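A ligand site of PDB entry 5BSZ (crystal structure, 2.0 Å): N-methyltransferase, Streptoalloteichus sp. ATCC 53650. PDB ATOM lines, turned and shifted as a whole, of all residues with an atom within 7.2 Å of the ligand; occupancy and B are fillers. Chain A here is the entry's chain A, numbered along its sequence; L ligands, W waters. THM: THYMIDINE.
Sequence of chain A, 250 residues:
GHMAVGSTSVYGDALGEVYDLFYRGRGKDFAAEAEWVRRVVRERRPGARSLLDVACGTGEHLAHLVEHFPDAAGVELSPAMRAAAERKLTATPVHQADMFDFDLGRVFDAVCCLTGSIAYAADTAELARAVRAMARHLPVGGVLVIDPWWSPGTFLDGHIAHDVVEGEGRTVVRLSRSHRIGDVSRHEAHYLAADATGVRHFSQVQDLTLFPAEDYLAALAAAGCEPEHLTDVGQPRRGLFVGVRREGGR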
ATOM      1  N   TRP A 149      11.963 -24.091 -17.843  1.00  0.00           N
ATOM      2  CA  TRP A 149      13.251 -24.319 -17.158  1.00  0.00           C
ATOM      3  C   TRP A 149      14.332 -24.110 -18.225  1.00  0.00           C
ATOM      4  O   TRP A 149      14.004 -23.837 -19.424  1.00  0.00           O
ATOM      5  CB  TRP A 149      13.269 -25.744 -16.580  1.00  0.00           C
ATOM      6  CG  TRP A 149      14.525 -26.093 -15.815  1.00  0.00           C
ATOM      7  CD1 TRP A 149      15.361 -27.136 -16.102  1.00  0.00           C
ATOM      8  CD2 TRP A 149      15.124 -25.398 -14.713  1.00  0.00           C
ATOM      9  NE1 TRP A 149      16.407 -27.146 -15.235  1.00  0.00           N
ATOM     10  CE2 TRP A 149      16.303 -26.084 -14.381  1.00  0.00           C
ATOM     11  CE3 TRP A 149      14.774 -24.292 -13.959  1.00  0.00           C
ATOM     12  CZ2 TRP A 149      17.136 -25.678 -13.338  1.00  0.00           C
ATOM     13  CZ3 TRP A 149      15.599 -23.903 -12.902  1.00  0.00           C
ATOM     14  CH2 TRP A 149      16.790 -24.586 -12.628  1.00  0.00           C
ATOM     15  N   TRP A 150      15.599 -24.172 -17.783  1.00  0.00           N
ATOM     16  CA  TRP A 150      16.764 -24.081 -18.664  1.00  0.00           C
ATOM     17  C   TRP A 150      16.821 -25.153 -19.725  1.00  0.00           C
ATOM     18  O   TRP A 150      16.188 -26.203 -19.606  1.00  0.00           O
ATOM     19  CB  TRP A 150      18.084 -23.951 -17.873  1.00  0.00           C
ATOM     20  CG  TRP A 150      18.034 -22.815 -16.880  1.00  0.00           C
ATOM     21  CD1 TRP A 150      17.806 -22.921 -15.508  1.00  0.00           C
ATOM     22  CD2 TRP A 150      18.145 -21.425 -17.154  1.00  0.00           C
ATOM     23  NE1 TRP A 150      17.786 -21.649 -14.926  1.00  0.00           N
ATOM     24  CE2 TRP A 150      18.009 -20.723 -15.913  1.00  0.00           C
ATOM     25  CE3 TRP A 150      18.367 -20.676 -18.328  1.00  0.00           C
ATOM     26  CZ2 TRP A 150      18.054 -19.318 -15.852  1.00  0.00           C
ATOM     27  CZ3 TRP A 150      18.449 -19.284 -18.248  1.00  0.00           C
ATOM     28  CH2 TRP A 150      18.290 -18.631 -17.019  1.00  0.00           C
ATOM     29  N   SER A 151      17.531 -24.827 -20.826  1.00  0.00           N
ATOM     30  CA  SER A 151      17.742 -25.731 -21.950  1.00  0.00           C
ATOM     31  C   SER A 151      19.134 -26.331 -21.839  1.00  0.00           C
ATOM     32  O   SER A 151      19.966 -25.808 -21.110  1.00  0.00           O
ATOM     33  CB  SER A 151      17.658 -24.880 -23.236  1.00  0.00           C
ATOM     34  OG  SER A 151      16.276 -24.577 -23.513  1.00  0.00           O
ATOM     35  N   THR A 154      21.629 -23.439 -22.158  1.00  0.00           N
ATOM     36  CA  THR A 154      21.628 -22.353 -21.215  1.00  0.00           C
ATOM     37  C   THR A 154      21.827 -22.793 -19.770  1.00  0.00           C
ATOM     38  O   THR A 154      22.093 -21.973 -18.920  1.00  0.00           O
ATOM     39  CB  THR A 154      20.354 -21.488 -21.356  1.00  0.00           C
ATOM     40  OG1 THR A 154      19.189 -22.324 -21.341  1.00  0.00           O
ATOM     41  CG2 THR A 154      20.378 -20.717 -22.724  1.00  0.00           C
ATOM     42  N   PHE A 155      21.690 -24.077 -19.468  1.00  0.00           N
ATOM     43  CA  PHE A 155      21.948 -24.510 -18.099  1.00  0.00           C
ATOM     44  C   PHE A 155      23.414 -24.295 -17.793  1.00  0.00           C
ATOM     45  O   PHE A 155      24.267 -24.613 -18.610  1.00  0.00           O
ATOM     46  CB  PHE A 155      21.565 -25.973 -17.914  1.00  0.00           C
ATOM     47  CG  PHE A 155      21.844 -26.489 -16.540  1.00  0.00           C
ATOM     48  CD1 PHE A 155      21.005 -26.133 -15.473  1.00  0.00           C
ATOM     49  CD2 PHE A 155      22.966 -27.234 -16.280  1.00  0.00           C
ATOM     50  CE1 PHE A 155      21.278 -26.555 -14.185  1.00  0.00           C
ATOM     51  CE2 PHE A 155      23.219 -27.704 -14.994  1.00  0.00           C
ATOM     52  CZ  PHE A 155      22.384 -27.359 -13.939  1.00  0.00           C
ATOM     53  N   LEU A 156      23.703 -23.766 -16.613  1.00  0.00           N
ATOM     54  CA  LEU A 156      25.070 -23.430 -16.219  1.00  0.00           C
ATOM     55  C   LEU A 156      25.499 -24.417 -15.167  1.00  0.00           C
ATOM     56  O   LEU A 156      24.878 -24.509 -14.159  1.00  0.00           O
ATOM     57  CB  LEU A 156      25.124 -22.015 -15.616  1.00  0.00           C
ATOM     58  CG  LEU A 156      24.814 -20.953 -16.673  1.00  0.00           C
ATOM     59  CD1 LEU A 156      24.849 -19.572 -16.019  1.00  0.00           C
ATOM     60  CD2 LEU A 156      25.704 -21.078 -17.936  1.00  0.00           C
ATOM     61  N   ASP A 157      26.581 -25.136 -15.427  1.00  0.00           N
ATOM     62  CA  ASP A 157      27.208 -26.024 -14.463  1.00  0.00           C
ATOM     63  C   ASP A 157      27.840 -25.153 -13.379  1.00  0.00           C
ATOM     64  O   ASP A 157      28.123 -23.973 -13.594  1.00  0.00           O
ATOM     65  CB  ASP A 157      28.277 -26.841 -15.208  1.00  0.00           C
ATOM     66  CG  ASP A 157      27.730 -27.455 -16.493  1.00  0.00           C
ATOM     67  OD1 ASP A 157      26.869 -28.341 -16.335  1.00  0.00           O
ATOM     68  OD2 ASP A 157      28.080 -27.045 -17.641  1.00  0.00           O
ATOM     69  N   GLY A 158      28.008 -25.711 -12.197  1.00  0.00           N
ATOM     70  CA  GLY A 158      28.699 -25.049 -11.097  1.00  0.00           C
ATOM     71  C   GLY A 158      27.826 -24.251 -10.137  1.00  0.00           C
ATOM     72  O   GLY A 158      28.337 -23.497  -9.325  1.00  0.00           O
ATOM     73  N   HIS A 159      26.499 -24.364 -10.199  1.00  0.00           N
ATOM     74  CA  HIS A 159      25.708 -23.534  -9.324  1.00  0.00           C
ATOM     75  C   HIS A 159      25.767 -24.066  -7.867  1.00  0.00           C
ATOM     76  O   HIS A 159      25.560 -25.255  -7.648  1.00  0.00           O
ATOM     77  CB  HIS A 159      24.274 -23.500  -9.767  1.00  0.00           C
ATOM     78  CG  HIS A 159      23.379 -22.742  -8.819  1.00  0.00           C
ATOM     79  ND1 HIS A 159      23.431 -21.373  -8.694  1.00  0.00           N
ATOM     80  CD2 HIS A 159      22.423 -23.156  -7.964  1.00  0.00           C
ATOM     81  CE1 HIS A 159      22.547 -20.974  -7.794  1.00  0.00           C
ATOM     82  NE2 HIS A 159      21.917 -22.039  -7.344  1.00  0.00           N
ATOM     83  N   ILE A 160      26.010 -23.163  -6.914  1.00  0.00           N
ATOM     84  CA  ILE A 160      25.993 -23.473  -5.466  1.00  0.00           C
ATOM     85  C   ILE A 160      25.398 -22.263  -4.836  1.00  0.00           C
ATOM     86  O   ILE A 160      25.788 -21.178  -5.185  1.00  0.00           O
ATOM     87  CB  ILE A 160      27.400 -23.674  -4.880  1.00  0.00           C
ATOM     88  CG1 ILE A 160      27.993 -24.931  -5.465  1.00  0.00           C
ATOM     89  CG2 ILE A 160      27.318 -23.736  -3.339  1.00  0.00           C
ATOM     90  CD1 ILE A 160      29.478 -25.091  -5.380  1.00  0.00           C
ATOM     91  N   ALA A 161      24.458 -22.422  -3.931  1.00  0.00           N
ATOM     92  CA  ALA A 161      23.844 -21.317  -3.248  1.00  0.00           C
ATOM     93  C   ALA A 161      23.626 -21.659  -1.777  1.00  0.00           C
ATOM     94  O   ALA A 161      23.519 -22.823  -1.447  1.00  0.00           O
ATOM     95  CB  ALA A 161      22.493 -21.005  -3.880  1.00  0.00           C
ATOM     96  N   SER A 176      22.573 -25.454  -1.369  1.00  0.00           N
ATOM     97  CA  SER A 176      22.041 -26.132  -2.528  1.00  0.00           C
ATOM     98  C   SER A 176      23.113 -26.236  -3.604  1.00  0.00           C
ATOM     99  O   SER A 176      24.038 -25.420  -3.646  1.00  0.00           O
ATOM    100  CB  SER A 176      20.789 -25.385  -2.995  1.00  0.00           C
ATOM    101  OG  SER A 176      21.152 -24.236  -3.732  1.00  0.00           O
ATOM    102  N   ARG A 177      22.974 -27.216  -4.476  1.00  0.00           N
ATOM    103  CA  ARG A 177      23.947 -27.515  -5.499  1.00  0.00           C
ATOM    104  C   ARG A 177      23.201 -28.124  -6.654  1.00  0.00           C
ATOM    105  O   ARG A 177      22.222 -28.837  -6.425  1.00  0.00           O
ATOM    106  CB  ARG A 177      24.886 -28.561  -4.991  1.00  0.00           C
ATOM    107  CG  ARG A 177      26.032 -28.793  -5.899  1.00  0.00           C
ATOM    108  CD  ARG A 177      26.773 -29.997  -5.418  1.00  0.00           C
ATOM    109  NE  ARG A 177      27.740 -30.346  -6.437  1.00  0.00           N
ATOM    110  CZ  ARG A 177      27.701 -31.449  -7.162  1.00  0.00           C
ATOM    111  NH1 ARG A 177      28.654 -31.644  -8.051  1.00  0.00           N
ATOM    112  NH2 ARG A 177      26.759 -32.365  -7.004  1.00  0.00           N
ATOM    113  N   SER A 178      23.633 -27.863  -7.894  1.00  0.00           N
ATOM    114  CA  SER A 178      23.006 -28.508  -9.062  1.00  0.00           C
ATOM    115  C   SER A 178      24.060 -29.027 -10.034  1.00  0.00           C
ATOM    116  O   SER A 178      25.161 -28.499 -10.091  1.00  0.00           O
ATOM    117  CB  SER A 178      21.977 -27.583  -9.704  1.00  0.00           C
ATOM    118  OG  SER A 178      22.572 -26.605 -10.555  1.00  0.00           O
ATOM    119  N   HIS A 179      23.747 -30.084 -10.763  1.00  0.00           N
ATOM    120  CA  HIS A 179      24.614 -30.574 -11.815  1.00  0.00           C
ATOM    121  C   HIS A 179      23.798 -31.268 -12.888  1.00  0.00           C
ATOM    122  O   HIS A 179      22.647 -31.688 -12.698  1.00  0.00           O
ATOM    123  CB  HIS A 179      25.706 -31.519 -11.314  1.00  0.00           C
ATOM    124  CG  HIS A 179      25.242 -32.871 -10.876  1.00  0.00           C
ATOM    125  ND1 HIS A 179      24.678 -33.094  -9.630  1.00  0.00           N
ATOM    126  CD2 HIS A 179      25.348 -34.073 -11.460  1.00  0.00           C
ATOM    127  CE1 HIS A 179      24.387 -34.361  -9.517  1.00  0.00           C
ATOM    128  NE2 HIS A 179      24.745 -34.981 -10.629  1.00  0.00           N
ATOM    129  N   SER A 185      18.830 -31.724 -15.211  1.00  0.00           N
ATOM    130  CA  SER A 185      19.578 -31.061 -14.132  1.00  0.00           C
ATOM    131  C   SER A 185      19.088 -31.660 -12.786  1.00  0.00           C
ATOM    132  O   SER A 185      17.907 -31.914 -12.600  1.00  0.00           O
ATOM    133  CB  SER A 185      19.418 -29.555 -14.168  1.00  0.00           C
ATOM    134  OG  SER A 185      18.043 -29.116 -14.109  1.00  0.00           O
ATOM    135  N   ARG A 186      20.043 -32.024 -11.950  1.00  0.00           N
ATOM    136  CA  ARG A 186      19.792 -32.619 -10.662  1.00  0.00           C
ATOM    137  C   ARG A 186      20.127 -31.648  -9.575  1.00  0.00           C
ATOM    138  O   ARG A 186      21.250 -31.112  -9.490  1.00  0.00           O
ATOM    139  CB  ARG A 186      20.619 -33.890 -10.500  1.00  0.00           C
ATOM    140  CG  ARG A 186      20.433 -34.571  -9.171  1.00  0.00           C
ATOM    141  CD  ARG A 186      20.785 -36.053  -9.294  1.00  0.00           C
ATOM    142  NE  ARG A 186      19.790 -36.802 -10.074  1.00  0.00           N
ATOM    143  CZ  ARG A 186      19.864 -38.087 -10.333  1.00  0.00           C
ATOM    144  NH1 ARG A 186      20.888 -38.794  -9.888  1.00  0.00           N
ATOM    145  NH2 ARG A 186      18.878 -38.692 -10.948  1.00  0.00           N
ATOM    146  N   HIS A 187      19.139 -31.392  -8.749  1.00  0.00           N
ATOM    147  CA  HIS A 187      19.192 -30.319  -7.740  1.00  0.00           C
ATOM    148  C   HIS A 187      19.215 -30.900  -6.331  1.00  0.00           C
ATOM    149  O   HIS A 187      18.302 -31.638  -5.912  1.00  0.00           O
ATOM    150  CB  HIS A 187      17.975 -29.375  -7.937  1.00  0.00           C
ATOM    151  CG  HIS A 187      18.004 -28.714  -9.271  1.00  0.00           C
ATOM    152  ND1 HIS A 187      18.513 -27.450  -9.467  1.00  0.00           N
ATOM    153  CD2 HIS A 187      17.664 -29.189 -10.498  1.00  0.00           C
ATOM    154  CE1 HIS A 187      18.485 -27.173 -10.758  1.00  0.00           C
ATOM    155  NE2 HIS A 187      17.980 -28.209 -11.404  1.00  0.00           N
ATOM    156  N   LEU A 210      16.054 -30.773 -19.150  1.00  0.00           N
ATOM    157  CA  LEU A 210      16.521 -29.694 -19.955  1.00  0.00           C
ATOM    158  C   LEU A 210      15.995 -29.837 -21.389  1.00  0.00           C
ATOM    159  O   LEU A 210      16.490 -30.691 -22.151  1.00  0.00           O
ATOM    160  CB  LEU A 210      18.054 -29.651 -19.916  1.00  0.00           C
ATOM    161  CG  LEU A 210      18.694 -29.547 -18.536  1.00  0.00           C
ATOM    162  CD1 LEU A 210      20.205 -29.849 -18.553  1.00  0.00           C
ATOM    163  CD2 LEU A 210      18.413 -28.171 -17.976  1.00  0.00           C
ATOM    164  N   GLN A 235      13.168 -14.720 -17.448  1.00  0.00           N
ATOM    165  CA  GLN A 235      14.561 -14.569 -17.049  1.00  0.00           C
ATOM    166  C   GLN A 235      15.426 -14.365 -18.290  1.00  0.00           C
ATOM    167  O   GLN A 235      15.073 -14.841 -19.406  1.00  0.00           O
ATOM    168  CB  GLN A 235      15.013 -15.800 -16.233  1.00  0.00           C
ATOM    169  CG  GLN A 235      14.159 -16.025 -14.984  1.00  0.00           C
ATOM    170  CD  GLN A 235      14.766 -16.901 -13.906  1.00  0.00           C
ATOM    171  OE1 GLN A 235      14.048 -17.542 -13.093  1.00  0.00           O
ATOM    172  NE2 GLN A 235      16.082 -16.908 -13.847  1.00  0.00           N
ATOM    173  N   PRO A 236      16.519 -13.616 -18.115  1.00  0.00           N
ATOM    174  CA  PRO A 236      17.483 -13.465 -19.211  1.00  0.00           C
ATOM    175  C   PRO A 236      17.971 -14.813 -19.722  1.00  0.00           C
ATOM    176  O   PRO A 236      18.213 -15.704 -18.922  1.00  0.00           O
ATOM    177  CB  PRO A 236      18.633 -12.675 -18.556  1.00  0.00           C
ATOM    178  CG  PRO A 236      17.920 -11.836 -17.561  1.00  0.00           C
ATOM    179  CD  PRO A 236      16.886 -12.757 -16.984  1.00  0.00           C
ATOM    180  N   ARG A 237      18.029 -14.934 -21.045  1.00  0.00           N
ATOM    181  CA  ARG A 237      18.545 -16.071 -21.775  1.00  0.00           C
ATOM    182  C   ARG A 237      17.542 -17.199 -21.718  1.00  0.00           C
ATOM    183  O   ARG A 237      17.741 -18.253 -22.319  1.00  0.00           O
ATOM    184  CB  ARG A 237      19.912 -16.546 -21.263  1.00  0.00           C
ATOM    185  CG  ARG A 237      20.945 -15.474 -20.956  1.00  0.00           C
ATOM    186  CD  ARG A 237      22.351 -16.014 -21.206  1.00  0.00           C
ATOM    187  NE  ARG A 237      22.596 -17.196 -20.388  1.00  0.00           N
ATOM    188  CZ  ARG A 237      23.326 -18.259 -20.720  1.00  0.00           C
ATOM    189  NH1 ARG A 237      23.409 -19.254 -19.836  1.00  0.00           N
ATOM    190  NH2 ARG A 237      23.995 -18.346 -21.869  1.00  0.00           N
ATOM    191  N   ARG A 238      16.420 -17.047 -21.030  1.00  0.00           N
ATOM    192  CA  ARG A 238      15.393 -18.030 -21.363  1.00  0.00           C
ATOM    193  C   ARG A 238      14.052 -17.585 -21.820  1.00  0.00           C
ATOM    194  O   ARG A 238      13.425 -18.281 -22.590  1.00  0.00           O
ATOM    195  CB  ARG A 238      15.209 -19.128 -20.311  1.00  0.00           C
ATOM    196  CG  ARG A 238      14.957 -18.683 -18.923  1.00  0.00           C
ATOM    197  CD  ARG A 238      14.815 -19.953 -18.064  1.00  0.00           C
ATOM    198  NE  ARG A 238      13.789 -19.588 -17.066  1.00  0.00           N
ATOM    199  CZ  ARG A 238      13.674 -20.032 -15.823  1.00  0.00           C
ATOM    200  NH1 ARG A 238      14.567 -20.870 -15.324  1.00  0.00           N
ATOM    201  NH2 ARG A 238      12.613 -19.665 -15.122  1.00  0.00           N
HETATM  202  O5' THM L   1      18.492 -20.663  -9.649  1.00  0.00           O
HETATM  203  C5' THM L   1      19.739 -21.369  -9.705  1.00  0.00           C
HETATM  204  C4' THM L   1      19.762 -22.392 -10.851  1.00  0.00           C
HETATM  205  O4' THM L   1      19.707 -21.543 -11.998  1.00  0.00           O
HETATM  206  C3' THM L   1      21.031 -23.260 -11.007  1.00  0.00           C
HETATM  207  O3' THM L   1      20.733 -24.676 -10.993  1.00  0.00           O
HETATM  208  C2' THM L   1      21.719 -22.877 -12.337  1.00  0.00           C
HETATM  209  C1' THM L   1      20.603 -22.043 -12.997  1.00  0.00           C
HETATM  210  N1  THM L   1      20.918 -20.943 -13.927  1.00  0.00           N
HETATM  211  C2  THM L   1      21.191 -21.453 -15.203  1.00  0.00           C
HETATM  212  O2  THM L   1      21.194 -22.685 -15.298  1.00  0.00           O
HETATM  213  N3  THM L   1      21.461 -20.680 -16.258  1.00  0.00           N
HETATM  214  C4  THM L   1      21.433 -19.353 -16.155  1.00  0.00           C
HETATM  215  O4  THM L   1      21.670 -18.624 -17.164  1.00  0.00           O
HETATM  216  C5  THM L   1      21.124 -18.794 -14.825  1.00  0.00           C
HETATM  217  C5M THM L   1      21.128 -17.283 -14.772  1.00  0.00           C
HETATM  218  C6  THM L   1      20.848 -19.614 -13.735  1.00  0.00           C
HETATM  219  O   HOH W   1      17.162 -20.620 -12.388  1.00  0.00           O
HETATM  220  O   HOH W   2      17.987 -18.203 -12.553  1.00  0.00           O
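Water W1 bridges O4' of the ligand (2.7 Å) and NE1 of Trp 150 (2.8 Å).
NE1 of Trp 150 lies close to N1 of the ligand. Residues that only touch the ligand: Phe 155, His 159 and His 187. Hydrophobic or aromatic side chains that line the ligand: Trp 150, Phe 155, Leu 156, His 159 and His 187. Within 4 Å of the ligand: Trp 150, Thr 154, Phe 155, Leu 156, His 159, Ser 178, His 187 and Arg 237.
The backbone NH (N) of Ser 178 sits at hydrogen-bond distance from the backbone carbonyl oxygen (O) of His 159 (3.3 Å). The backbone carbonyl oxygen of Thr 154 is in hydrogen-bond range of the guanidinium group of Arg 237 (3.2 Å). OG1 of Thr 154 is in hydrogen-bond range of N of Ser 151 (3.0 Å). A ring nitrogen (NE2) of His 187 is in hydrogen-bond range of the side-chain hydroxyl (OG) of Ser 185 (2.9 Å).
The side-chain hydroxyl (OG) of Ser 178 lies within hydrogen-bond range of an oxygen (O3') of the ligand, at 2.7 Å. The backbone carbonyl oxygen (O) of Thr 154 lies within hydrogen-bond range of a nitrogen (N3) of the ligand. An oxygen (O2) of the ligand lies within hydrogen-bond range of the backbone NH (N) of Leu 156 (3.0 Å). An oxygen (O4) of the ligand is in hydrogen-bond range of the guanidinium group of Arg 237 (3.2 Å).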
